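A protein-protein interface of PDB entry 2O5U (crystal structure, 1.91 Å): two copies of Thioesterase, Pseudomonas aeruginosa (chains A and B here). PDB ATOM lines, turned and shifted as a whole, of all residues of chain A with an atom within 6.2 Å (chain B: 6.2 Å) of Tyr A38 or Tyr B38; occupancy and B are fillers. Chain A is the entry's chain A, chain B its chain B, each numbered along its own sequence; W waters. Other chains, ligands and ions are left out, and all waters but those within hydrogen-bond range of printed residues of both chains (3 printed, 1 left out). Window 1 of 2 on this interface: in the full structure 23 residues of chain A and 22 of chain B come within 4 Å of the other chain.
Of the 18 printed residues of chain B, 11 touch a printed residue of chain A. Of the 18 printed residues of chain A, 11 touch a printed residue of chain B. Hydrophobic or aromatic side chains of chain A within 4 Å of the printed part of chain B: Val A35, Tyr A38 and Tyr A73. Along chain A the printed residues that touch a printed residue of chain B span positions 34 to 73.
Tyr A38 touches just these residues of chain B: Val B35, Tyr B38 and Ser B69. Tyr B38 touches just these residues of chain A: Val A35, Tyr A38 and Ser A69. Of the printed residues of chain B, Ser A68 touches Cys B71, Asp B72 and Tyr B73. Of the printed residues of chain B, Ser A69 touches Tyr B38 (2.8 Å), Ser B70 (3.2 Å), Cys B71 (3.0 Å) and Tyr B73 (3.6 Å). Of the printed residues of chain B, Asp A72 touches Ser B68. Phe A41 touches none of the printed residues of chain B. Arg A116 touches none of the printed residues of chain B. The nearest residue of chain B that does not touch Tyr A38 is Ser B70 (4.03 Å). The nearest residue of chain A that does not touch Tyr B38 is Ser A70 (4.1 Å).
Water W1 lies within hydrogen-bond range of OG of Ser B69 (2.6 Å), OD1 of Asn A34 (2.7 Å) and OH of Tyr A73 (3.0 Å). Water W3 bridges the side-chain amide nitrogen (ND2) of Asn B34 (2.7 Å) and the side-chain hydroxyl (OG) of Ser A69 (2.8 Å). Water W2 bridges OD2 of Asp A42 and OD1 of Asn B34.
C of Tyr B38 touches CG2 of Val A35, at 3.5 Å. Ala B39 touches Val A35 (N to CG2, 3.5 Å). Ala A39 touches Val B35 (N to CG2, 3.6 Å). Ser A68 touches Cys B71 (CA to O, 3.2 Å). OD1 of Asp B72 touches CB of Ser A68, at 3.4 Å. N of Ser A68 touches CD1 of Tyr B73 (3.8 Å). Ser B70 touches Ser A69. Ser A70 touches Ser B69 (CA to O, 3.3 Å). CA of Ser B68 touches O of Cys A71 (3.3 Å). Ser B68 touches Asp A72 (CB to OD1, 3.5 Å).
Val B35 touches its own counterpart, Val A35. Tyr B38 touches its own counterpart, Tyr A38. Tyr A38 touches Ser B69, and with the chains exchanged Ser A69 touches Tyr B38. Asp A42 touches Val B35, but with the chains exchanged Val A35 does not touch Asp B42 (4.2 Å). 18 positions are printed for both chains. Of the 24 pairs that touch across the chains among the printed residues, 23 have their exchanged pair printed and touching as well.
The side-chain carboxylate (OD2) of Asp B42 is in hydrogen-bond range of the side-chain amide nitrogen (ND2) of Asn A34 (3.1 Å). OH of Tyr B38 sits at hydrogen-bond distance from OH of Tyr A38. OG of Ser B69 sits at hydrogen-bond distance from OH of Tyr A38 (2.8 Å). The side-chain amide oxygen of Asn B34 lies close to the side-chain carboxylate of Asp A42, at 3.2 Å. OH of Tyr B38 is in hydrogen-bond range of OG of Ser A69, 2.8 Å away. O of Ser A69 is in hydrogen-bond range of N of Cys B71 (3.0 Å). N of Cys A71 lies within hydrogen-bond range of O of Ser B69, at 3.0 Å.
The side-chain hydroxyl (OH) of Tyr A38 sits at hydrogen-bond distance from the backbone NH (N) of Cys A71 (3.0 Å). The backbone carbonyl oxygen of Ala A39 sits at hydrogen-bond distance from the side-chain hydroxyl of Thr A43, at 2.8 Å. N of Arg A116 is in hydrogen-bond range of O of Ser A70, 2.8 Å away. O of Asn B34 sits at hydrogen-bond distance from OH of Tyr B73, 2.8 Å away. The side-chain hydroxyl (OG1) of Thr B43 lies within hydrogen-bond range of the backbone carbonyl oxygen (O) of Ala B39. The backbone carbonyl oxygen of Ser B70 is in hydrogen-bond range of the backbone NH of Arg B116 (3.0 Å).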
ATOM      1  N   ASN A  34      16.863 -19.918  28.202  1.00  0.00           N
ATOM      2  CA  ASN A  34      17.009 -21.288  28.741  1.00  0.00           C
ATOM      3  C   ASN A  34      18.113 -22.172  28.092  1.00  0.00           C
ATOM      4  O   ASN A  34      18.813 -22.926  28.769  1.00  0.00           O
ATOM      5  CB  ASN A  34      15.643 -22.003  28.647  1.00  0.00           C
ATOM      6  CG  ASN A  34      15.163 -22.209  27.200  1.00  0.00           C
ATOM      7  OD1 ASN A  34      15.347 -23.278  26.610  1.00  0.00           O
ATOM      8  ND2 ASN A  34      14.574 -21.190  26.630  1.00  0.00           N
ATOM      9  N   VAL A  35      18.273 -22.061  26.773  1.00  0.00           N
ATOM     10  CA  VAL A  35      19.292 -22.841  26.017  1.00  0.00           C
ATOM     11  C   VAL A  35      20.726 -22.540  26.524  1.00  0.00           C
ATOM     12  O   VAL A  35      21.598 -23.450  26.635  1.00  0.00           O
ATOM     13  CB  VAL A  35      19.145 -22.584  24.502  1.00  0.00           C
ATOM     14  CG1 VAL A  35      20.327 -23.300  23.678  1.00  0.00           C
ATOM     15  CG2 VAL A  35      17.749 -23.114  24.062  1.00  0.00           C
ATOM     16  N   THR A  36      20.949 -21.261  26.818  1.00  0.00           N
ATOM     17  CA  THR A  36      22.262 -20.738  27.203  1.00  0.00           C
ATOM     18  C   THR A  36      22.804 -21.436  28.426  1.00  0.00           C
ATOM     19  O   THR A  36      23.981 -21.614  28.547  1.00  0.00           O
ATOM     20  CB  THR A  36      22.248 -19.167  27.377  1.00  0.00           C
ATOM     21  OG1 THR A  36      21.630 -18.560  26.226  1.00  0.00           O
ATOM     22  CG2 THR A  36      23.680 -18.577  27.517  1.00  0.00           C
ATOM     23  N   TYR A  37      21.925 -21.892  29.298  1.00  0.00           N
ATOM     24  CA  TYR A  37      22.354 -22.548  30.516  1.00  0.00           C
ATOM     25  C   TYR A  37      23.109 -23.828  30.196  1.00  0.00           C
ATOM     26  O   TYR A  37      24.112 -24.150  30.835  1.00  0.00           O
ATOM     27  CB  TYR A  37      21.133 -22.834  31.381  1.00  0.00           C
ATOM     28  CG  TYR A  37      20.603 -21.600  32.104  1.00  0.00           C
ATOM     29  CD1 TYR A  37      19.810 -20.677  31.427  1.00  0.00           C
ATOM     30  CD2 TYR A  37      20.924 -21.362  33.440  1.00  0.00           C
ATOM     31  CE1 TYR A  37      19.307 -19.529  32.059  1.00  0.00           C
ATOM     32  CE2 TYR A  37      20.421 -20.226  34.110  1.00  0.00           C
ATOM     33  CZ  TYR A  37      19.612 -19.331  33.427  1.00  0.00           C
ATOM     34  OH  TYR A  37      19.116 -18.237  34.105  1.00  0.00           O
ATOM     35  N   TYR A  38      22.676 -24.531  29.153  1.00  0.00           N
ATOM     36  CA  TYR A  38      23.385 -25.746  28.756  1.00  0.00           C
ATOM     37  C   TYR A  38      24.765 -25.475  28.199  1.00  0.00           C
ATOM     38  O   TYR A  38      25.681 -26.294  28.352  1.00  0.00           O
ATOM     39  CB  TYR A  38      22.544 -26.534  27.748  1.00  0.00           C
ATOM     40  CG  TYR A  38      21.302 -27.148  28.333  1.00  0.00           C
ATOM     41  CD1 TYR A  38      20.040 -26.629  28.046  1.00  0.00           C
ATOM     42  CD2 TYR A  38      21.388 -28.258  29.172  1.00  0.00           C
ATOM     43  CE1 TYR A  38      18.899 -27.197  28.604  1.00  0.00           C
ATOM     44  CE2 TYR A  38      20.260 -28.834  29.741  1.00  0.00           C
ATOM     45  CZ  TYR A  38      19.019 -28.325  29.429  1.00  0.00           C
ATOM     46  OH  TYR A  38      17.906 -28.931  29.985  1.00  0.00           O
ATOM     47  N   ALA A  39      24.915 -24.343  27.521  1.00  0.00           N
ATOM     48  CA  ALA A  39      26.227 -23.841  27.102  1.00  0.00           C
ATOM     49  C   ALA A  39      27.132 -23.513  28.300  1.00  0.00           C
ATOM     50  O   ALA A  39      28.328 -23.841  28.269  1.00  0.00           O
ATOM     51  CB  ALA A  39      26.099 -22.652  26.154  1.00  0.00           C
ATOM     52  N   PHE A  40      26.560 -22.928  29.357  1.00  0.00           N
ATOM     53  CA  PHE A  40      27.297 -22.773  30.645  1.00  0.00           C
ATOM     54  C   PHE A  40      27.693 -24.157  31.230  1.00  0.00           C
ATOM     55  O   PHE A  40      28.818 -24.300  31.718  1.00  0.00           O
ATOM     56  CB  PHE A  40      26.475 -22.012  31.698  1.00  0.00           C
ATOM     57  CG  PHE A  40      26.095 -20.611  31.287  1.00  0.00           C
ATOM     58  CD1 PHE A  40      26.938 -19.855  30.467  1.00  0.00           C
ATOM     59  CD2 PHE A  40      24.947 -20.020  31.782  1.00  0.00           C
ATOM     60  CE1 PHE A  40      26.601 -18.531  30.127  1.00  0.00           C
ATOM     61  CE2 PHE A  40      24.589 -18.666  31.405  1.00  0.00           C
ATOM     62  CZ  PHE A  40      25.418 -17.960  30.604  1.00  0.00           C
ATOM     63  N   PHE A  41      26.791 -25.148  31.207  1.00  0.00           N
ATOM     64  CA  PHE A  41      27.127 -26.497  31.756  1.00  0.00           C
ATOM     65  C   PHE A  41      28.355 -27.089  30.959  1.00  0.00           C
ATOM     66  O   PHE A  41      29.315 -27.616  31.534  1.00  0.00           O
ATOM     67  CB  PHE A  41      25.982 -27.456  31.518  1.00  0.00           C
ATOM     68  CG  PHE A  41      24.731 -27.240  32.381  1.00  0.00           C
ATOM     69  CD1 PHE A  41      24.614 -26.195  33.292  1.00  0.00           C
ATOM     70  CD2 PHE A  41      23.687 -28.171  32.290  1.00  0.00           C
ATOM     71  CE1 PHE A  41      23.445 -26.050  34.080  1.00  0.00           C
ATOM     72  CE2 PHE A  41      22.528 -28.048  33.083  1.00  0.00           C
ATOM     73  CZ  PHE A  41      22.401 -26.983  33.969  1.00  0.00           C
ATOM     74  N   ASP A  42      28.283 -27.011  29.640  1.00  0.00           N
ATOM     75  CA  ASP A  42      29.306 -27.537  28.735  1.00  0.00           C
ATOM     76  C   ASP A  42      30.644 -26.869  28.962  1.00  0.00           C
ATOM     77  O   ASP A  42      31.726 -27.539  28.945  1.00  0.00           O
ATOM     78  CB  ASP A  42      28.925 -27.248  27.252  1.00  0.00           C
ATOM     79  CG  ASP A  42      28.146 -28.360  26.613  1.00  0.00           C
ATOM     80  OD1 ASP A  42      27.511 -29.141  27.366  1.00  0.00           O
ATOM     81  OD2 ASP A  42      28.186 -28.462  25.366  1.00  0.00           O
ATOM     82  N   THR A  43      30.582 -25.545  29.115  1.00  0.00           N
ATOM     83  CA  THR A  43      31.754 -24.729  29.398  1.00  0.00           C
ATOM     84  C   THR A  43      32.400 -25.047  30.727  1.00  0.00           C
ATOM     85  O   THR A  43      33.600 -25.252  30.780  1.00  0.00           O
ATOM     86  CB  THR A  43      31.414 -23.206  29.266  1.00  0.00           C
ATOM     87  OG1 THR A  43      30.970 -23.029  27.929  1.00  0.00           O
ATOM     88  CG2 THR A  43      32.652 -22.319  29.560  1.00  0.00           C
ATOM     89  N   SER A  68      22.774 -37.417  27.651  1.00  0.00           N
ATOM     90  CA  SER A  68      21.520 -36.900  28.198  1.00  0.00           C
ATOM     91  C   SER A  68      21.834 -35.620  28.997  1.00  0.00           C
ATOM     92  O   SER A  68      22.964 -35.449  29.488  1.00  0.00           O
ATOM     93  CB  SER A  68      20.916 -37.966  29.097  1.00  0.00           C
ATOM     94  OG  SER A  68      21.913 -38.342  30.066  1.00  0.00           O
ATOM     95  N   SER A  69      20.851 -34.722  29.157  1.00  0.00           N
ATOM     96  CA  SER A  69      21.052 -33.574  29.982  1.00  0.00           C
ATOM     97  C   SER A  69      19.681 -33.121  30.435  1.00  0.00           C
ATOM     98  O   SER A  69      18.649 -33.515  29.857  1.00  0.00           O
ATOM     99  CB  SER A  69      21.742 -32.417  29.233  1.00  0.00           C
ATOM    100  OG  SER A  69      21.079 -32.135  27.972  1.00  0.00           O
ATOM    101  N   SER A  70      19.674 -32.316  31.462  1.00  0.00           N
ATOM    102  CA  SER A  70      18.406 -31.667  31.879  1.00  0.00           C
ATOM    103  C   SER A  70      18.673 -30.450  32.731  1.00  0.00           C
ATOM    104  O   SER A  70      19.805 -30.287  33.304  1.00  0.00           O
ATOM    105  CB  SER A  70      17.496 -32.678  32.612  1.00  0.00           C
ATOM    106  OG  SER A  70      18.169 -33.225  33.743  1.00  0.00           O
ATOM    107  N   CYS A  71      17.660 -29.570  32.861  1.00  0.00           N
ATOM    108  CA  CYS A  71      17.822 -28.370  33.682  1.00  0.00           C
ATOM    109  C   CYS A  71      16.476 -27.951  34.262  1.00  0.00           C
ATOM    110  O   CYS A  71      15.446 -28.099  33.607  1.00  0.00           O
ATOM    111  CB  CYS A  71      18.346 -27.188  32.825  1.00  0.00           C
ATOM    112  SG  CYS A  71      18.989 -25.772  33.772  1.00  0.00           S
ATOM    113  N   ASP A  72      16.504 -27.430  35.483  1.00  0.00           N
ATOM    114  CA  ASP A  72      15.341 -26.747  36.091  1.00  0.00           C
ATOM    115  C   ASP A  72      15.725 -25.313  36.273  1.00  0.00           C
ATOM    116  O   ASP A  72      16.827 -25.009  36.712  1.00  0.00           O
ATOM    117  CB  ASP A  72      14.984 -27.366  37.460  1.00  0.00           C
ATOM    118  CG  ASP A  72      14.585 -28.835  37.339  1.00  0.00           C
ATOM    119  OD1 ASP A  72      13.571 -29.141  36.687  1.00  0.00           O
ATOM    120  OD2 ASP A  72      15.327 -29.689  37.866  1.00  0.00           O
ATOM    121  N   TYR A  73      14.821 -24.413  35.950  1.00  0.00           N
ATOM    122  CA  TYR A  73      15.083 -22.972  36.033  1.00  0.00           C
ATOM    123  C   TYR A  73      14.232 -22.371  37.146  1.00  0.00           C
ATOM    124  O   TYR A  73      12.993 -22.427  37.063  1.00  0.00           O
ATOM    125  CB  TYR A  73      14.711 -22.339  34.710  1.00  0.00           C
ATOM    126  CG  TYR A  73      15.426 -22.966  33.518  1.00  0.00           C
ATOM    127  CD1 TYR A  73      14.910 -24.084  32.863  1.00  0.00           C
ATOM    128  CD2 TYR A  73      16.639 -22.432  33.076  1.00  0.00           C
ATOM    129  CE1 TYR A  73      15.615 -24.700  31.756  1.00  0.00           C
ATOM    130  CE2 TYR A  73      17.318 -22.988  31.973  1.00  0.00           C
ATOM    131  CZ  TYR A  73      16.814 -24.112  31.341  1.00  0.00           C
ATOM    132  OH  TYR A  73      17.526 -24.589  30.268  1.00  0.00           O
ATOM    133  N   ARG A 116      21.755 -31.330  35.060  1.00  0.00           N
ATOM    134  CA  ARG A 116      22.736 -32.434  35.045  1.00  0.00           C
ATOM    135  C   ARG A 116      23.057 -32.783  33.629  1.00  0.00           C
ATOM    136  O   ARG A 116      22.305 -32.446  32.728  1.00  0.00           O
ATOM    137  CB  ARG A 116      22.208 -33.687  35.785  1.00  0.00           C
ATOM    138  CG  ARG A 116      20.847 -34.192  35.376  1.00  0.00           C
ATOM    139  CD  ARG A 116      20.315 -35.187  36.439  1.00  0.00           C
ATOM    140  N   PHE A 117      24.174 -33.454  33.418  1.00  0.00           N
ATOM    141  CA  PHE A 117      24.353 -34.118  32.155  1.00  0.00           C
ATOM    142  C   PHE A 117      25.337 -35.260  32.278  1.00  0.00           C
ATOM    143  O   PHE A 117      26.116 -35.284  33.227  1.00  0.00           O
ATOM    144  CB  PHE A 117      24.692 -33.127  31.014  1.00  0.00           C
ATOM    145  CG  PHE A 117      26.126 -32.696  30.917  1.00  0.00           C
ATOM    146  CD1 PHE A 117      27.053 -33.454  30.154  1.00  0.00           C
ATOM    147  CD2 PHE A 117      26.560 -31.511  31.539  1.00  0.00           C
ATOM    148  CE1 PHE A 117      28.403 -33.030  29.993  1.00  0.00           C
ATOM    149  CE2 PHE A 117      27.881 -31.075  31.399  1.00  0.00           C
ATOM    150  CZ  PHE A 117      28.830 -31.849  30.612  1.00  0.00           C
ATOM    151  N   ASN B  34      25.161 -30.755  21.525  1.00  0.00           N
ATOM    152  CA  ASN B  34      24.014 -31.041  22.382  1.00  0.00           C
ATOM    153  C   ASN B  34      23.139 -29.841  22.730  1.00  0.00           C
ATOM    154  O   ASN B  34      21.904 -29.926  22.722  1.00  0.00           O
ATOM    155  CB  ASN B  34      24.480 -31.765  23.665  1.00  0.00           C
ATOM    156  CG  ASN B  34      25.557 -30.995  24.396  1.00  0.00           C
ATOM    157  OD1 ASN B  34      26.720 -31.009  24.012  1.00  0.00           O
ATOM    158  ND2 ASN B  34      25.158 -30.287  25.423  1.00  0.00           N
ATOM    159  N   VAL B  35      23.771 -28.709  22.998  1.00  0.00           N
ATOM    160  CA  VAL B  35      23.058 -27.448  23.345  1.00  0.00           C
ATOM    161  C   VAL B  35      22.037 -27.047  22.250  1.00  0.00           C
ATOM    162  O   VAL B  35      20.885 -26.626  22.514  1.00  0.00           O
ATOM    163  CB  VAL B  35      24.078 -26.317  23.649  1.00  0.00           C
ATOM    164  CG1 VAL B  35      23.363 -24.862  23.825  1.00  0.00           C
ATOM    165  CG2 VAL B  35      24.964 -26.701  24.823  1.00  0.00           C
ATOM    166  N   THR B  36      22.407 -27.292  20.992  1.00  0.00           N
ATOM    167  CA  THR B  36      21.665 -26.741  19.842  1.00  0.00           C
ATOM    168  C   THR B  36      20.318 -27.414  19.796  1.00  0.00           C
ATOM    169  O   THR B  36      19.376 -26.864  19.232  1.00  0.00           O
ATOM    170  CB  THR B  36      22.476 -26.970  18.520  1.00  0.00           C
ATOM    171  OG1 THR B  36      23.731 -26.365  18.713  1.00  0.00           O
ATOM    172  CG2 THR B  36      21.819 -26.245  17.272  1.00  0.00           C
ATOM    173  N   TYR B  37      20.198 -28.617  20.392  1.00  0.00           N
ATOM    174  CA  TYR B  37      18.927 -29.340  20.298  1.00  0.00           C
ATOM    175  C   TYR B  37      17.874 -28.553  21.064  1.00  0.00           C
ATOM    176  O   TYR B  37      16.678 -28.520  20.702  1.00  0.00           O
ATOM    177  CB  TYR B  37      19.053 -30.783  20.808  1.00  0.00           C
ATOM    178  CG  TYR B  37      19.855 -31.721  19.861  1.00  0.00           C
ATOM    179  CD1 TYR B  37      21.257 -31.607  19.705  1.00  0.00           C
ATOM    180  CD2 TYR B  37      19.196 -32.733  19.132  1.00  0.00           C
ATOM    181  CE1 TYR B  37      21.970 -32.503  18.880  1.00  0.00           C
ATOM    182  CE2 TYR B  37      19.928 -33.631  18.280  1.00  0.00           C
ATOM    183  CZ  TYR B  37      21.281 -33.490  18.168  1.00  0.00           C
ATOM    184  OH  TYR B  37      21.926 -34.361  17.357  1.00  0.00           O
ATOM    185  N   TYR B  38      18.286 -27.920  22.147  1.00  0.00           N
ATOM    186  CA  TYR B  38      17.300 -27.135  22.931  1.00  0.00           C
ATOM    187  C   TYR B  38      16.863 -25.890  22.184  1.00  0.00           C
ATOM    188  O   TYR B  38      15.729 -25.449  22.316  1.00  0.00           O
ATOM    189  CB  TYR B  38      17.928 -26.779  24.222  1.00  0.00           C
ATOM    190  CG  TYR B  38      18.092 -27.973  25.125  1.00  0.00           C
ATOM    191  CD1 TYR B  38      19.329 -28.623  25.263  1.00  0.00           C
ATOM    192  CD2 TYR B  38      16.998 -28.489  25.806  1.00  0.00           C
ATOM    193  CE1 TYR B  38      19.483 -29.735  26.141  1.00  0.00           C
ATOM    194  CE2 TYR B  38      17.121 -29.602  26.655  1.00  0.00           C
ATOM    195  CZ  TYR B  38      18.384 -30.209  26.815  1.00  0.00           C
ATOM    196  OH  TYR B  38      18.472 -31.267  27.660  1.00  0.00           O
ATOM    197  N   ALA B  39      17.745 -25.336  21.340  1.00  0.00           N
ATOM    198  CA  ALA B  39      17.365 -24.231  20.472  1.00  0.00           C
ATOM    199  C   ALA B  39      16.316 -24.693  19.455  1.00  0.00           C
ATOM    200  O   ALA B  39      15.397 -23.955  19.114  1.00  0.00           O
ATOM    201  CB  ALA B  39      18.589 -23.668  19.751  1.00  0.00           C
ATOM    202  N   PHE B  40      16.489 -25.902  18.922  1.00  0.00           N
ATOM    203  CA  PHE B  40      15.472 -26.520  18.042  1.00  0.00           C
ATOM    204  C   PHE B  40      14.155 -26.716  18.755  1.00  0.00           C
ATOM    205  O   PHE B  40      13.119 -26.508  18.155  1.00  0.00           O
ATOM    206  CB  PHE B  40      15.912 -27.902  17.557  1.00  0.00           C
ATOM    207  CG  PHE B  40      17.150 -27.889  16.698  1.00  0.00           C
ATOM    208  CD1 PHE B  40      17.503 -26.775  15.928  1.00  0.00           C
ATOM    209  CD2 PHE B  40      17.935 -29.062  16.597  1.00  0.00           C
ATOM    210  CE1 PHE B  40      18.688 -26.803  15.099  1.00  0.00           C
ATOM    211  CE2 PHE B  40      19.093 -29.086  15.797  1.00  0.00           C
ATOM    212  CZ  PHE B  40      19.447 -27.933  15.030  1.00  0.00           C
ATOM    213  N   PHE B  41      14.197 -27.158  20.011  1.00  0.00           N
ATOM    214  CA  PHE B  41      12.966 -27.296  20.806  1.00  0.00           C
ATOM    215  C   PHE B  41      12.280 -25.922  20.957  1.00  0.00           C
ATOM    216  O   PHE B  41      11.076 -25.798  20.757  1.00  0.00           O
ATOM    217  CB  PHE B  41      13.266 -27.817  22.228  1.00  0.00           C
ATOM    218  CG  PHE B  41      13.699 -29.251  22.297  1.00  0.00           C
ATOM    219  CD1 PHE B  41      13.869 -30.015  21.174  1.00  0.00           C
ATOM    220  CD2 PHE B  41      13.970 -29.819  23.565  1.00  0.00           C
ATOM    221  CE1 PHE B  41      14.355 -31.350  21.274  1.00  0.00           C
ATOM    222  CE2 PHE B  41      14.392 -31.103  23.671  1.00  0.00           C
ATOM    223  CZ  PHE B  41      14.609 -31.860  22.522  1.00  0.00           C
ATOM    224  N   ASP B  42      13.058 -24.926  21.359  1.00  0.00           N
ATOM    225  CA  ASP B  42      12.499 -23.550  21.566  1.00  0.00           C
ATOM    226  C   ASP B  42      11.856 -23.019  20.285  1.00  0.00           C
ATOM    227  O   ASP B  42      10.859 -22.304  20.294  1.00  0.00           O
ATOM    228  CB  ASP B  42      13.647 -22.594  21.914  1.00  0.00           C
ATOM    229  CG  ASP B  42      13.617 -22.082  23.343  1.00  0.00           C
ATOM    230  OD1 ASP B  42      13.084 -22.792  24.225  1.00  0.00           O
ATOM    231  OD2 ASP B  42      14.194 -20.991  23.606  1.00  0.00           O
ATOM    232  N   THR B  43      12.515 -23.296  19.166  1.00  0.00           N
ATOM    233  CA  THR B  43      12.133 -22.731  17.871  1.00  0.00           C
ATOM    234  C   THR B  43      10.882 -23.423  17.349  1.00  0.00           C
ATOM    235  O   THR B  43       9.986 -22.768  16.827  1.00  0.00           O
ATOM    236  CB  THR B  43      13.286 -22.942  16.908  1.00  0.00           C
ATOM    237  OG1 THR B  43      14.364 -22.102  17.309  1.00  0.00           O
ATOM    238  CG2 THR B  43      12.879 -22.648  15.436  1.00  0.00           C
ATOM    239  N   SER B  68      11.610 -25.923  32.813  1.00  0.00           N
ATOM    240  CA  SER B  68      12.443 -27.142  32.810  1.00  0.00           C
ATOM    241  C   SER B  68      12.555 -27.738  31.429  1.00  0.00           C
ATOM    242  O   SER B  68      11.698 -27.465  30.543  1.00  0.00           O
ATOM    243  CB  SER B  68      11.886 -28.155  33.820  1.00  0.00           C
ATOM    244  OG  SER B  68      10.704 -28.700  33.319  1.00  0.00           O
ATOM    245  N   SER B  69      13.611 -28.542  31.208  1.00  0.00           N
ATOM    246  CA  SER B  69      13.798 -29.190  29.917  1.00  0.00           C
ATOM    247  C   SER B  69      14.750 -30.385  30.081  1.00  0.00           C
ATOM    248  O   SER B  69      15.473 -30.475  31.099  1.00  0.00           O
ATOM    249  CB  SER B  69      14.374 -28.271  28.857  1.00  0.00           C
ATOM    250  OG  SER B  69      15.530 -27.574  29.345  1.00  0.00           O
ATOM    251  N   SER B  70      14.750 -31.269  29.094  1.00  0.00           N
ATOM    252  CA  SER B  70      15.683 -32.430  29.142  1.00  0.00           C
ATOM    253  C   SER B  70      15.752 -33.000  27.746  1.00  0.00           C
ATOM    254  O   SER B  70      14.830 -32.804  26.959  1.00  0.00           O
ATOM    255  CB  SER B  70      15.220 -33.525  30.129  1.00  0.00           C
ATOM    256  OG  SER B  70      13.883 -33.932  29.840  1.00  0.00           O
ATOM    257  N   CYS B  71      16.832 -33.737  27.451  1.00  0.00           N
ATOM    258  CA  CYS B  71      16.995 -34.344  26.162  1.00  0.00           C
ATOM    259  C   CYS B  71      17.861 -35.609  26.309  1.00  0.00           C
ATOM    260  O   CYS B  71      18.809 -35.644  27.103  1.00  0.00           O
ATOM    261  CB  CYS B  71      17.737 -33.378  25.271  1.00  0.00           C
ATOM    262  SG  CYS B  71      17.651 -33.809  23.538  1.00  0.00           S
ATOM    263  N   ASP B  72      17.499 -36.634  25.566  1.00  0.00           N
ATOM    264  CA  ASP B  72      18.313 -37.850  25.471  1.00  0.00           C
ATOM    265  C   ASP B  72      18.816 -37.912  24.034  1.00  0.00           C
ATOM    266  O   ASP B  72      18.042 -37.719  23.084  1.00  0.00           O
ATOM    267  CB  ASP B  72      17.477 -39.076  25.799  1.00  0.00           C
ATOM    268  CG  ASP B  72      17.019 -39.127  27.270  1.00  0.00           C
ATOM    269  OD1 ASP B  72      17.818 -38.992  28.201  1.00  0.00           O
ATOM    270  OD2 ASP B  72      15.813 -39.255  27.487  1.00  0.00           O
ATOM    271  N   TYR B  73      20.107 -38.196  23.850  1.00  0.00           N
ATOM    272  CA  TYR B  73      20.669 -38.177  22.566  1.00  0.00           C
ATOM    273  C   TYR B  73      21.038 -39.597  22.138  1.00  0.00           C
ATOM    274  O   TYR B  73      21.852 -40.252  22.848  1.00  0.00           O
ATOM    275  CB  TYR B  73      21.931 -37.303  22.609  1.00  0.00           C
ATOM    276  CG  TYR B  73      21.688 -35.885  23.101  1.00  0.00           C
ATOM    277  CD1 TYR B  73      21.703 -35.574  24.477  1.00  0.00           C
ATOM    278  CD2 TYR B  73      21.429 -34.854  22.185  1.00  0.00           C
ATOM    279  CE1 TYR B  73      21.469 -34.201  24.932  1.00  0.00           C
ATOM    280  CE2 TYR B  73      21.206 -33.525  22.635  1.00  0.00           C
ATOM    281  CZ  TYR B  73      21.244 -33.234  24.005  1.00  0.00           C
ATOM    282  OH  TYR B  73      21.043 -31.939  24.412  1.00  0.00           O
ATOM    283  N   ARG B 116      11.930 -33.054  26.177  1.00  0.00           N
ATOM    284  CA  ARG B 116      10.695 -32.510  26.663  1.00  0.00           C
ATOM    285  C   ARG B 116      11.004 -31.135  27.176  1.00  0.00           C
ATOM    286  O   ARG B 116      12.157 -30.823  27.486  1.00  0.00           O
ATOM    287  CB  ARG B 116      10.088 -33.386  27.761  1.00  0.00           C
ATOM    288  CG  ARG B 116      10.720 -33.338  29.100  1.00  0.00           C
ATOM    289  CD  ARG B 116      10.116 -34.521  29.938  1.00  0.00           C
ATOM    290  N   PHE B 117      10.003 -30.260  27.189  1.00  0.00           N
ATOM    291  CA  PHE B 117      10.132 -29.036  27.985  1.00  0.00           C
ATOM    292  C   PHE B 117       8.813 -28.473  28.369  1.00  0.00           C
ATOM    293  O   PHE B 117       7.785 -28.885  27.838  1.00  0.00           O
ATOM    294  CB  PHE B 117      11.089 -28.015  27.388  1.00  0.00           C
ATOM    295  CG  PHE B 117      10.472 -27.038  26.428  1.00  0.00           C
ATOM    296  CD1 PHE B 117       9.755 -25.924  26.911  1.00  0.00           C
ATOM    297  CD2 PHE B 117      10.687 -27.149  25.109  1.00  0.00           C
ATOM    298  CE1 PHE B 117       9.217 -24.967  26.076  1.00  0.00           C
ATOM    299  CE2 PHE B 117      10.152 -26.180  24.222  1.00  0.00           C
ATOM    300  CZ  PHE B 117       9.399 -25.067  24.733  1.00  0.00           C
HETATM  301  O   HOH W   1      16.105 -25.613  27.811  1.00  0.00           O
HETATM  302  O   HOH W   2      29.528 -30.639  24.330  1.00  0.00           O
HETATM  303  O   HOH W   3      22.936 -30.350  26.906  1.00  0.00           O
